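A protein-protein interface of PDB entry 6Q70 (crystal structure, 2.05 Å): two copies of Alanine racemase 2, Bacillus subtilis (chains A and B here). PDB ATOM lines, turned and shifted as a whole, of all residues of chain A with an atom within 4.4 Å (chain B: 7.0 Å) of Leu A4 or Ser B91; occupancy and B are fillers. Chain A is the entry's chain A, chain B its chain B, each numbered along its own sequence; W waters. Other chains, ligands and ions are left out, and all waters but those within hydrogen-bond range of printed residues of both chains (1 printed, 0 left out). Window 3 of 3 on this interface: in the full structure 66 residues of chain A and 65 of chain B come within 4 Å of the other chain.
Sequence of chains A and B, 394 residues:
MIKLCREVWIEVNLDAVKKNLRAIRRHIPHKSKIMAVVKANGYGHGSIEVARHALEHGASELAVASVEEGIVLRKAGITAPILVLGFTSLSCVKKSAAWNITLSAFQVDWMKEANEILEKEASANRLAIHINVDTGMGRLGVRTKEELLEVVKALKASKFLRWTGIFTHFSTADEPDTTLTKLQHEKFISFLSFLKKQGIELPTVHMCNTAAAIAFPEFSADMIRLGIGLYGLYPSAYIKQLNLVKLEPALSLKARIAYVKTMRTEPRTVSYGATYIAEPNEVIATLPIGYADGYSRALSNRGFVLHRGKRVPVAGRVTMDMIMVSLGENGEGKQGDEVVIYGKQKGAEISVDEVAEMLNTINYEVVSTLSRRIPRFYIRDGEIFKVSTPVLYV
The side-chain carboxylate (OE1) of Glu B68 is in hydrogen-bond range of the backbone NH (N) of Cys A5 (3.2 Å).
The backbone carbonyl oxygen (O) of Cys A5 sits at hydrogen-bond distance from the backbone NH (N) of Ser B89, 3.1 Å away.
The side-chain sulfur of Cys A5 is disulfide-bonded to the side-chain sulfur of Cys B92, at 2.0 Å.
The side-chain sulfur (SG) of Cys A5 lies within hydrogen-bond range of the side-chain amino group (NZ) of Lys B95 (3.8 Å).
The indole nitrogen (NE1) of Trp B110 lies within hydrogen-bond range of the backbone carbonyl oxygen (O) of Thr B88.
OG of Ser B89 lies close to N of Ser B91.
O of Leu A4 touches CB of Ser B89 (3.2 Å).
O of Leu A4 touches CB of Ser B91, 3.99 Å away.
SG of Cys B92 touches C of Leu A4, 3.9 Å away.
Thr B88 touches Cys A5.
Glu B68 touches Arg A6 (OE2 to N, 3.6 Å).
Glu A7 touches Ser B89 (OE1 to OG, 3.5 Å).
Lys A3 touches none of the printed residues of chain B.
Printed residues of chain B within 4 Å of Leu A4: Ser B89 (3.2 Å), Ser B91 (3.99 Å) and Cys B92 (3.9 Å).
Of the printed residues of chain B, Cys A5 touches Glu B68, Thr B88, Ser B89, Cys B92 and Lys B95.
Printed residues of chain B within 4 Å of Arg A6: Glu B68 (3.6 Å).
Printed residues of chain B within 4 Å of Glu A7: Ser B89 (3.5 Å).
Trp A9 touches none of the printed residues of chain B.
Of the printed residues of chain A, Thr B88 touches Cys A5 (3.7 Å).
Of the printed residues of chain A, Ser B91 touches Leu A4 (3.99 Å).
Of the printed residues of chain A, Cys B92 touches Leu A4 and Cys A5.
The nearest printed residue of chain A that does not touch Ser B91 is Lys A3 (4.03 Å).
The nearest printed residue of chain A that does not touch Thr B88 is Arg A6 (5.4 Å).
Of the 11 printed residues of chain B, 6 touch a printed residue of chain A.
Of the 10 printed residues of chain A, 4 touch a printed residue of chain B.
Among the printed residues, 10 pairs touch across the chains.
No position is printed for both chains.
Of the 10 pairs that touch across the chains among the printed residues, none has its exchanged pair printed and touching as well.
Water W1 lies within hydrogen-bond range of N of Leu A4 (2.9 Å), OG of Ser B91 (3.0 Å), OE1 of Glu A7 (3.0 Å) and OG of Ser B89 (3.2 Å).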
ATOM      1  N   ILE A   2     -14.257  -3.851 -19.167  1.00  0.00           N
ATOM      2  CA  ILE A   2     -13.089  -4.311 -19.916  1.00  0.00           C
ATOM      3  C   ILE A   2     -12.680  -5.769 -19.619  1.00  0.00           C
ATOM      4  O   ILE A   2     -12.528  -6.092 -18.468  1.00  0.00           O
ATOM      5  CB  ILE A   2     -11.924  -3.368 -19.559  1.00  0.00           C
ATOM      6  CG1 ILE A   2     -12.192  -1.966 -20.162  1.00  0.00           C
ATOM      7  CG2 ILE A   2     -10.596  -3.906 -20.112  1.00  0.00           C
ATOM      8  CD1 ILE A   2     -11.359  -0.868 -19.547  1.00  0.00           C
ATOM      9  N   LYS A   3     -12.507  -6.616 -20.625  1.00  0.00           N
ATOM     10  CA  LYS A   3     -11.843  -7.944 -20.402  1.00  0.00           C
ATOM     11  C   LYS A   3     -10.330  -8.000 -20.759  1.00  0.00           C
ATOM     12  O   LYS A   3     -10.003  -7.776 -21.907  1.00  0.00           O
ATOM     13  CB  LYS A   3     -12.423  -9.014 -21.330  1.00  0.00           C
ATOM     14  CG  LYS A   3     -13.861  -9.410 -21.185  1.00  0.00           C
ATOM     15  CD  LYS A   3     -14.143 -10.291 -22.429  1.00  0.00           C
ATOM     16  CE  LYS A   3     -15.599 -10.649 -22.608  1.00  0.00           C
ATOM     17  NZ  LYS A   3     -16.164 -10.918 -21.265  1.00  0.00           N
ATOM     18  N   LEU A   4      -9.464  -8.409 -19.840  1.00  0.00           N
ATOM     19  CA  LEU A   4      -8.037  -8.573 -20.116  1.00  0.00           C
ATOM     20  C   LEU A   4      -7.478  -9.836 -19.457  1.00  0.00           C
ATOM     21  O   LEU A   4      -8.031 -10.311 -18.430  1.00  0.00           O
ATOM     22  CB  LEU A   4      -7.268  -7.399 -19.529  1.00  0.00           C
ATOM     23  CG  LEU A   4      -7.596  -6.106 -20.223  1.00  0.00           C
ATOM     24  CD1 LEU A   4      -7.108  -4.942 -19.404  1.00  0.00           C
ATOM     25  CD2 LEU A   4      -7.099  -6.103 -21.677  1.00  0.00           C
ATOM     26  N   CYS A   5      -6.398 -10.341 -20.019  1.00  0.00           N
ATOM     27  CA  CYS A   5      -5.675 -11.507 -19.342  1.00  0.00           C
ATOM     28  C   CYS A   5      -4.970 -11.068 -18.007  1.00  0.00           C
ATOM     29  O   CYS A   5      -5.392 -11.365 -16.849  1.00  0.00           O
ATOM     30  CB  CYS A   5      -4.803 -12.171 -20.349  1.00  0.00           C
ATOM     31  SG  CYS A   5      -5.659 -12.753 -21.843  1.00  0.00           S
ATOM     32  N   ARG A   6      -4.073 -10.149 -18.210  1.00  0.00           N
ATOM     33  CA  ARG A   6      -3.461  -9.353 -17.181  1.00  0.00           C
ATOM     34  C   ARG A   6      -4.198  -8.012 -17.053  1.00  0.00           C
ATOM     35  O   ARG A   6      -4.152  -7.196 -17.958  1.00  0.00           O
ATOM     36  CB  ARG A   6      -2.035  -9.062 -17.671  1.00  0.00           C
ATOM     37  CG  ARG A   6      -1.156  -8.420 -16.625  1.00  0.00           C
ATOM     38  CD  ARG A   6       0.147  -8.109 -17.236  1.00  0.00           C
ATOM     39  NE  ARG A   6       1.067  -7.600 -16.213  1.00  0.00           N
ATOM     40  CZ  ARG A   6       1.834  -6.524 -16.328  1.00  0.00           C
ATOM     41  NH1 ARG A   6       1.717  -5.706 -17.347  1.00  0.00           N
ATOM     42  NH2 ARG A   6       2.701  -6.224 -15.328  1.00  0.00           N
ATOM     43  N   GLU A   7      -4.682  -7.692 -15.852  1.00  0.00           N
ATOM     44  CA  GLU A   7      -5.703  -6.622 -15.656  1.00  0.00           C
ATOM     45  C   GLU A   7      -5.064  -5.313 -15.291  1.00  0.00           C
ATOM     46  O   GLU A   7      -5.210  -4.829 -14.190  1.00  0.00           O
ATOM     47  CB  GLU A   7      -6.726  -7.085 -14.596  1.00  0.00           C
ATOM     48  CG  GLU A   7      -7.341  -8.349 -15.099  1.00  0.00           C
ATOM     49  CD  GLU A   7      -8.475  -8.971 -14.216  1.00  0.00           C
ATOM     50  OE1 GLU A   7      -9.519  -9.196 -14.787  1.00  0.00           O
ATOM     51  OE2 GLU A   7      -8.307  -9.240 -13.041  1.00  0.00           O
ATOM     52  N   VAL A   8      -4.285  -4.728 -16.234  1.00  0.00           N
ATOM     53  CA  VAL A   8      -3.771  -3.379 -16.032  1.00  0.00           C
ATOM     54  C   VAL A   8      -4.015  -2.667 -17.344  1.00  0.00           C
ATOM     55  O   VAL A   8      -3.828  -3.282 -18.401  1.00  0.00           O
ATOM     56  CB  VAL A   8      -2.310  -3.347 -15.638  1.00  0.00           C
ATOM     57  CG1 VAL A   8      -1.458  -4.016 -16.716  1.00  0.00           C
ATOM     58  CG2 VAL A   8      -1.848  -1.913 -15.240  1.00  0.00           C
ATOM     59  N   TRP A   9      -4.498  -1.407 -17.273  1.00  0.00           N
ATOM     60  CA  TRP A   9      -4.825  -0.643 -18.426  1.00  0.00           C
ATOM     61  C   TRP A   9      -4.740   0.853 -18.181  1.00  0.00           C
ATOM     62  O   TRP A   9      -4.790   1.350 -17.062  1.00  0.00           O
ATOM     63  CB  TRP A   9      -6.220  -0.957 -18.972  1.00  0.00           C
ATOM     64  CG  TRP A   9      -7.383  -0.535 -18.146  1.00  0.00           C
ATOM     65  CD1 TRP A   9      -8.205   0.510 -18.369  1.00  0.00           C
ATOM     66  CD2 TRP A   9      -7.906  -1.217 -17.021  1.00  0.00           C
ATOM     67  NE1 TRP A   9      -9.197   0.548 -17.432  1.00  0.00           N
ATOM     68  CE2 TRP A   9      -9.021  -0.470 -16.568  1.00  0.00           C
ATOM     69  CE3 TRP A   9      -7.484  -2.368 -16.288  1.00  0.00           C
ATOM     70  CZ2 TRP A   9      -9.793  -0.834 -15.493  1.00  0.00           C
ATOM     71  CZ3 TRP A   9      -8.250  -2.741 -15.180  1.00  0.00           C
ATOM     72  CH2 TRP A   9      -9.417  -1.952 -14.807  1.00  0.00           C
ATOM     73  N   PRO A 375      -2.342  -1.911 -22.235  1.00  0.00           N
ATOM     74  CA  PRO A 375      -3.229  -1.503 -23.376  1.00  0.00           C
ATOM     75  C   PRO A 375      -3.876  -0.134 -23.065  1.00  0.00           C
ATOM     76  O   PRO A 375      -4.134   0.141 -21.909  1.00  0.00           O
ATOM     77  CB  PRO A 375      -4.277  -2.591 -23.394  1.00  0.00           C
ATOM     78  CG  PRO A 375      -4.391  -3.069 -21.962  1.00  0.00           C
ATOM     79  CD  PRO A 375      -2.950  -2.948 -21.384  1.00  0.00           C
ATOM     80  N   PHE A 377      -7.130   2.405 -23.614  1.00  0.00           N
ATOM     81  CA  PHE A 377      -8.537   2.571 -23.923  1.00  0.00           C
ATOM     82  C   PHE A 377      -8.796   4.088 -23.952  1.00  0.00           C
ATOM     83  O   PHE A 377      -8.228   4.846 -23.179  1.00  0.00           O
ATOM     84  CB  PHE A 377      -9.370   1.853 -22.817  1.00  0.00           C
ATOM     85  CG  PHE A 377      -9.202   0.371 -22.834  1.00  0.00           C
ATOM     86  CD1 PHE A 377      -8.216  -0.221 -22.091  1.00  0.00           C
ATOM     87  CD2 PHE A 377     -10.018  -0.444 -23.676  1.00  0.00           C
ATOM     88  CE1 PHE A 377      -8.011  -1.554 -22.171  1.00  0.00           C
ATOM     89  CE2 PHE A 377      -9.870  -1.812 -23.708  1.00  0.00           C
ATOM     90  CZ  PHE A 377      -8.837  -2.384 -22.950  1.00  0.00           C
ATOM     91  N   GLU B  68      -0.598 -12.368 -23.120  1.00  0.00           N
ATOM     92  CA  GLU B  68      -0.355 -11.619 -24.313  1.00  0.00           C
ATOM     93  C   GLU B  68       1.154 -11.768 -24.739  1.00  0.00           C
ATOM     94  O   GLU B  68       1.473 -11.961 -25.896  1.00  0.00           O
ATOM     95  CB  GLU B  68      -0.920 -10.123 -24.214  1.00  0.00           C
ATOM     96  CG  GLU B  68      -2.470  -9.881 -23.776  1.00  0.00           C
ATOM     97  CD  GLU B  68      -2.877  -9.759 -22.132  1.00  0.00           C
ATOM     98  OE1 GLU B  68      -3.942  -9.074 -21.671  1.00  0.00           O
ATOM     99  OE2 GLU B  68      -2.199 -10.351 -21.236  1.00  0.00           O
ATOM    100  N   THR B  88      -3.797 -14.752 -14.181  1.00  0.00           N
ATOM    101  CA  THR B  88      -4.514 -14.702 -15.433  1.00  0.00           C
ATOM    102  C   THR B  88      -5.983 -14.801 -15.089  1.00  0.00           C
ATOM    103  O   THR B  88      -6.441 -15.797 -14.520  1.00  0.00           O
ATOM    104  CB  THR B  88      -4.139 -15.834 -16.401  1.00  0.00           C
ATOM    105  OG1 THR B  88      -2.746 -15.729 -16.754  1.00  0.00           O
ATOM    106  CG2 THR B  88      -4.987 -15.730 -17.683  1.00  0.00           C
ATOM    107  N   SER B  89      -6.705 -13.747 -15.452  1.00  0.00           N
ATOM    108  CA  SER B  89      -8.148 -13.659 -15.321  1.00  0.00           C
ATOM    109  C   SER B  89      -8.884 -14.821 -15.936  1.00  0.00           C
ATOM    110  O   SER B  89      -8.505 -15.261 -17.033  1.00  0.00           O
ATOM    111  CB  SER B  89      -8.567 -12.373 -16.029  1.00  0.00           C
ATOM    112  OG  SER B  89      -9.924 -12.365 -16.223  1.00  0.00           O
ATOM    113  N   LEU B  90      -9.980 -15.289 -15.286  1.00  0.00           N
ATOM    114  CA  LEU B  90     -10.812 -16.333 -15.879  1.00  0.00           C
ATOM    115  C   LEU B  90     -11.341 -16.020 -17.268  1.00  0.00           C
ATOM    116  O   LEU B  90     -11.559 -16.943 -18.091  1.00  0.00           O
ATOM    117  CB  LEU B  90     -11.998 -16.758 -14.931  1.00  0.00           C
ATOM    118  CG  LEU B  90     -11.535 -17.479 -13.679  1.00  0.00           C
ATOM    119  CD1 LEU B  90     -12.621 -17.613 -12.557  1.00  0.00           C
ATOM    120  CD2 LEU B  90     -11.058 -18.861 -14.037  1.00  0.00           C
ATOM    121  N   SER B  91     -11.499 -14.723 -17.535  1.00  0.00           N
ATOM    122  CA  SER B  91     -11.695 -14.156 -18.906  1.00  0.00           C
ATOM    123  C   SER B  91     -10.879 -14.799 -19.977  1.00  0.00           C
ATOM    124  O   SER B  91     -11.355 -14.851 -21.094  1.00  0.00           O
ATOM    125  CB  SER B  91     -11.163 -12.720 -19.006  1.00  0.00           C
ATOM    126  OG  SER B  91     -12.142 -11.929 -18.555  1.00  0.00           O
ATOM    127  N   CYS B  92      -9.608 -15.087 -19.683  1.00  0.00           N
ATOM    128  CA  CYS B  92      -8.641 -15.592 -20.712  1.00  0.00           C
ATOM    129  C   CYS B  92      -8.384 -17.043 -20.718  1.00  0.00           C
ATOM    130  O   CYS B  92      -7.456 -17.507 -21.451  1.00  0.00           O
ATOM    131  CB  CYS B  92      -7.232 -14.994 -20.552  1.00  0.00           C
ATOM    132  SG  CYS B  92      -7.412 -13.386 -21.047  1.00  0.00           S
ATOM    133  N   VAL B  93      -9.176 -17.775 -19.967  1.00  0.00           N
ATOM    134  CA  VAL B  93      -8.913 -19.196 -19.906  1.00  0.00           C
ATOM    135  C   VAL B  93      -8.997 -19.850 -21.310  1.00  0.00           C
ATOM    136  O   VAL B  93      -8.162 -20.681 -21.685  1.00  0.00           O
ATOM    137  CB  VAL B  93      -9.919 -19.838 -18.945  1.00  0.00           C
ATOM    138  CG1 VAL B  93     -10.103 -21.232 -19.340  1.00  0.00           C
ATOM    139  CG2 VAL B  93      -9.372 -19.760 -17.526  1.00  0.00           C
ATOM    140  N   LYS B  94     -10.047 -19.502 -22.047  1.00  0.00           N
ATOM    141  CA  LYS B  94     -10.348 -20.108 -23.289  1.00  0.00           C
ATOM    142  C   LYS B  94      -9.231 -19.718 -24.272  1.00  0.00           C
ATOM    143  O   LYS B  94      -8.630 -20.535 -24.927  1.00  0.00           O
ATOM    144  CB  LYS B  94     -11.726 -19.614 -23.696  1.00  0.00           C
ATOM    145  CG  LYS B  94     -12.170 -20.105 -25.049  1.00  0.00           C
ATOM    146  CD  LYS B  94     -13.660 -19.805 -25.259  1.00  0.00           C
ATOM    147  CE  LYS B  94     -13.878 -18.326 -25.614  1.00  0.00           C
ATOM    148  NZ  LYS B  94     -13.889 -18.197 -27.097  1.00  0.00           N
ATOM    149  N   LYS B  95      -8.861 -18.472 -24.222  1.00  0.00           N
ATOM    150  CA  LYS B  95      -7.842 -17.986 -25.139  1.00  0.00           C
ATOM    151  C   LYS B  95      -6.466 -18.673 -24.891  1.00  0.00           C
ATOM    152  O   LYS B  95      -5.697 -18.913 -25.846  1.00  0.00           O
ATOM    153  CB  LYS B  95      -7.773 -16.494 -24.951  1.00  0.00           C
ATOM    154  CG  LYS B  95      -6.699 -15.810 -25.767  1.00  0.00           C
ATOM    155  CD  LYS B  95      -6.428 -14.387 -25.322  1.00  0.00           C
ATOM    156  CE  LYS B  95      -7.586 -13.504 -25.615  1.00  0.00           C
ATOM    157  NZ  LYS B  95      -7.049 -12.125 -25.300  1.00  0.00           N
ATOM    158  N   TRP B 110     -10.768 -20.724  -8.696  1.00  0.00           N
ATOM    159  CA  TRP B 110     -10.173 -20.538  -9.990  1.00  0.00           C
ATOM    160  C   TRP B 110     -10.075 -21.837 -10.790  1.00  0.00           C
ATOM    161  O   TRP B 110     -10.631 -21.811 -11.900  1.00  0.00           O
ATOM    162  CB  TRP B 110      -8.809 -19.864  -9.866  1.00  0.00           C
ATOM    163  CG  TRP B 110      -8.343 -19.296 -11.103  1.00  0.00           C
ATOM    164  CD1 TRP B 110      -8.438 -18.034 -11.469  1.00  0.00           C
ATOM    165  CD2 TRP B 110      -7.686 -19.986 -12.187  1.00  0.00           C
ATOM    166  NE1 TRP B 110      -7.863 -17.831 -12.715  1.00  0.00           N
ATOM    167  CE2 TRP B 110      -7.385 -19.019 -13.174  1.00  0.00           C
ATOM    168  CE3 TRP B 110      -7.314 -21.316 -12.411  1.00  0.00           C
ATOM    169  CZ2 TRP B 110      -6.765 -19.342 -14.382  1.00  0.00           C
ATOM    170  CZ3 TRP B 110      -6.700 -21.629 -13.571  1.00  0.00           C
ATOM    171  CH2 TRP B 110      -6.442 -20.652 -14.573  1.00  0.00           C
ATOM    172  N   ILE B 117     -15.571 -23.361 -17.776  1.00  0.00           N
ATOM    173  CA  ILE B 117     -15.446 -22.582 -19.065  1.00  0.00           C
ATOM    174  C   ILE B 117     -14.985 -23.540 -20.206  1.00  0.00           C
ATOM    175  O   ILE B 117     -15.623 -23.632 -21.295  1.00  0.00           O
ATOM    176  CB  ILE B 117     -14.495 -21.378 -18.946  1.00  0.00           C
ATOM    177  CG1 ILE B 117     -15.037 -20.319 -17.972  1.00  0.00           C
ATOM    178  CG2 ILE B 117     -14.303 -20.706 -20.288  1.00  0.00           C
ATOM    179  CD1 ILE B 117     -13.914 -19.395 -17.453  1.00  0.00           C
HETATM  180  O   HOH W   1     -10.805  -9.520 -17.470  1.00  0.00           O
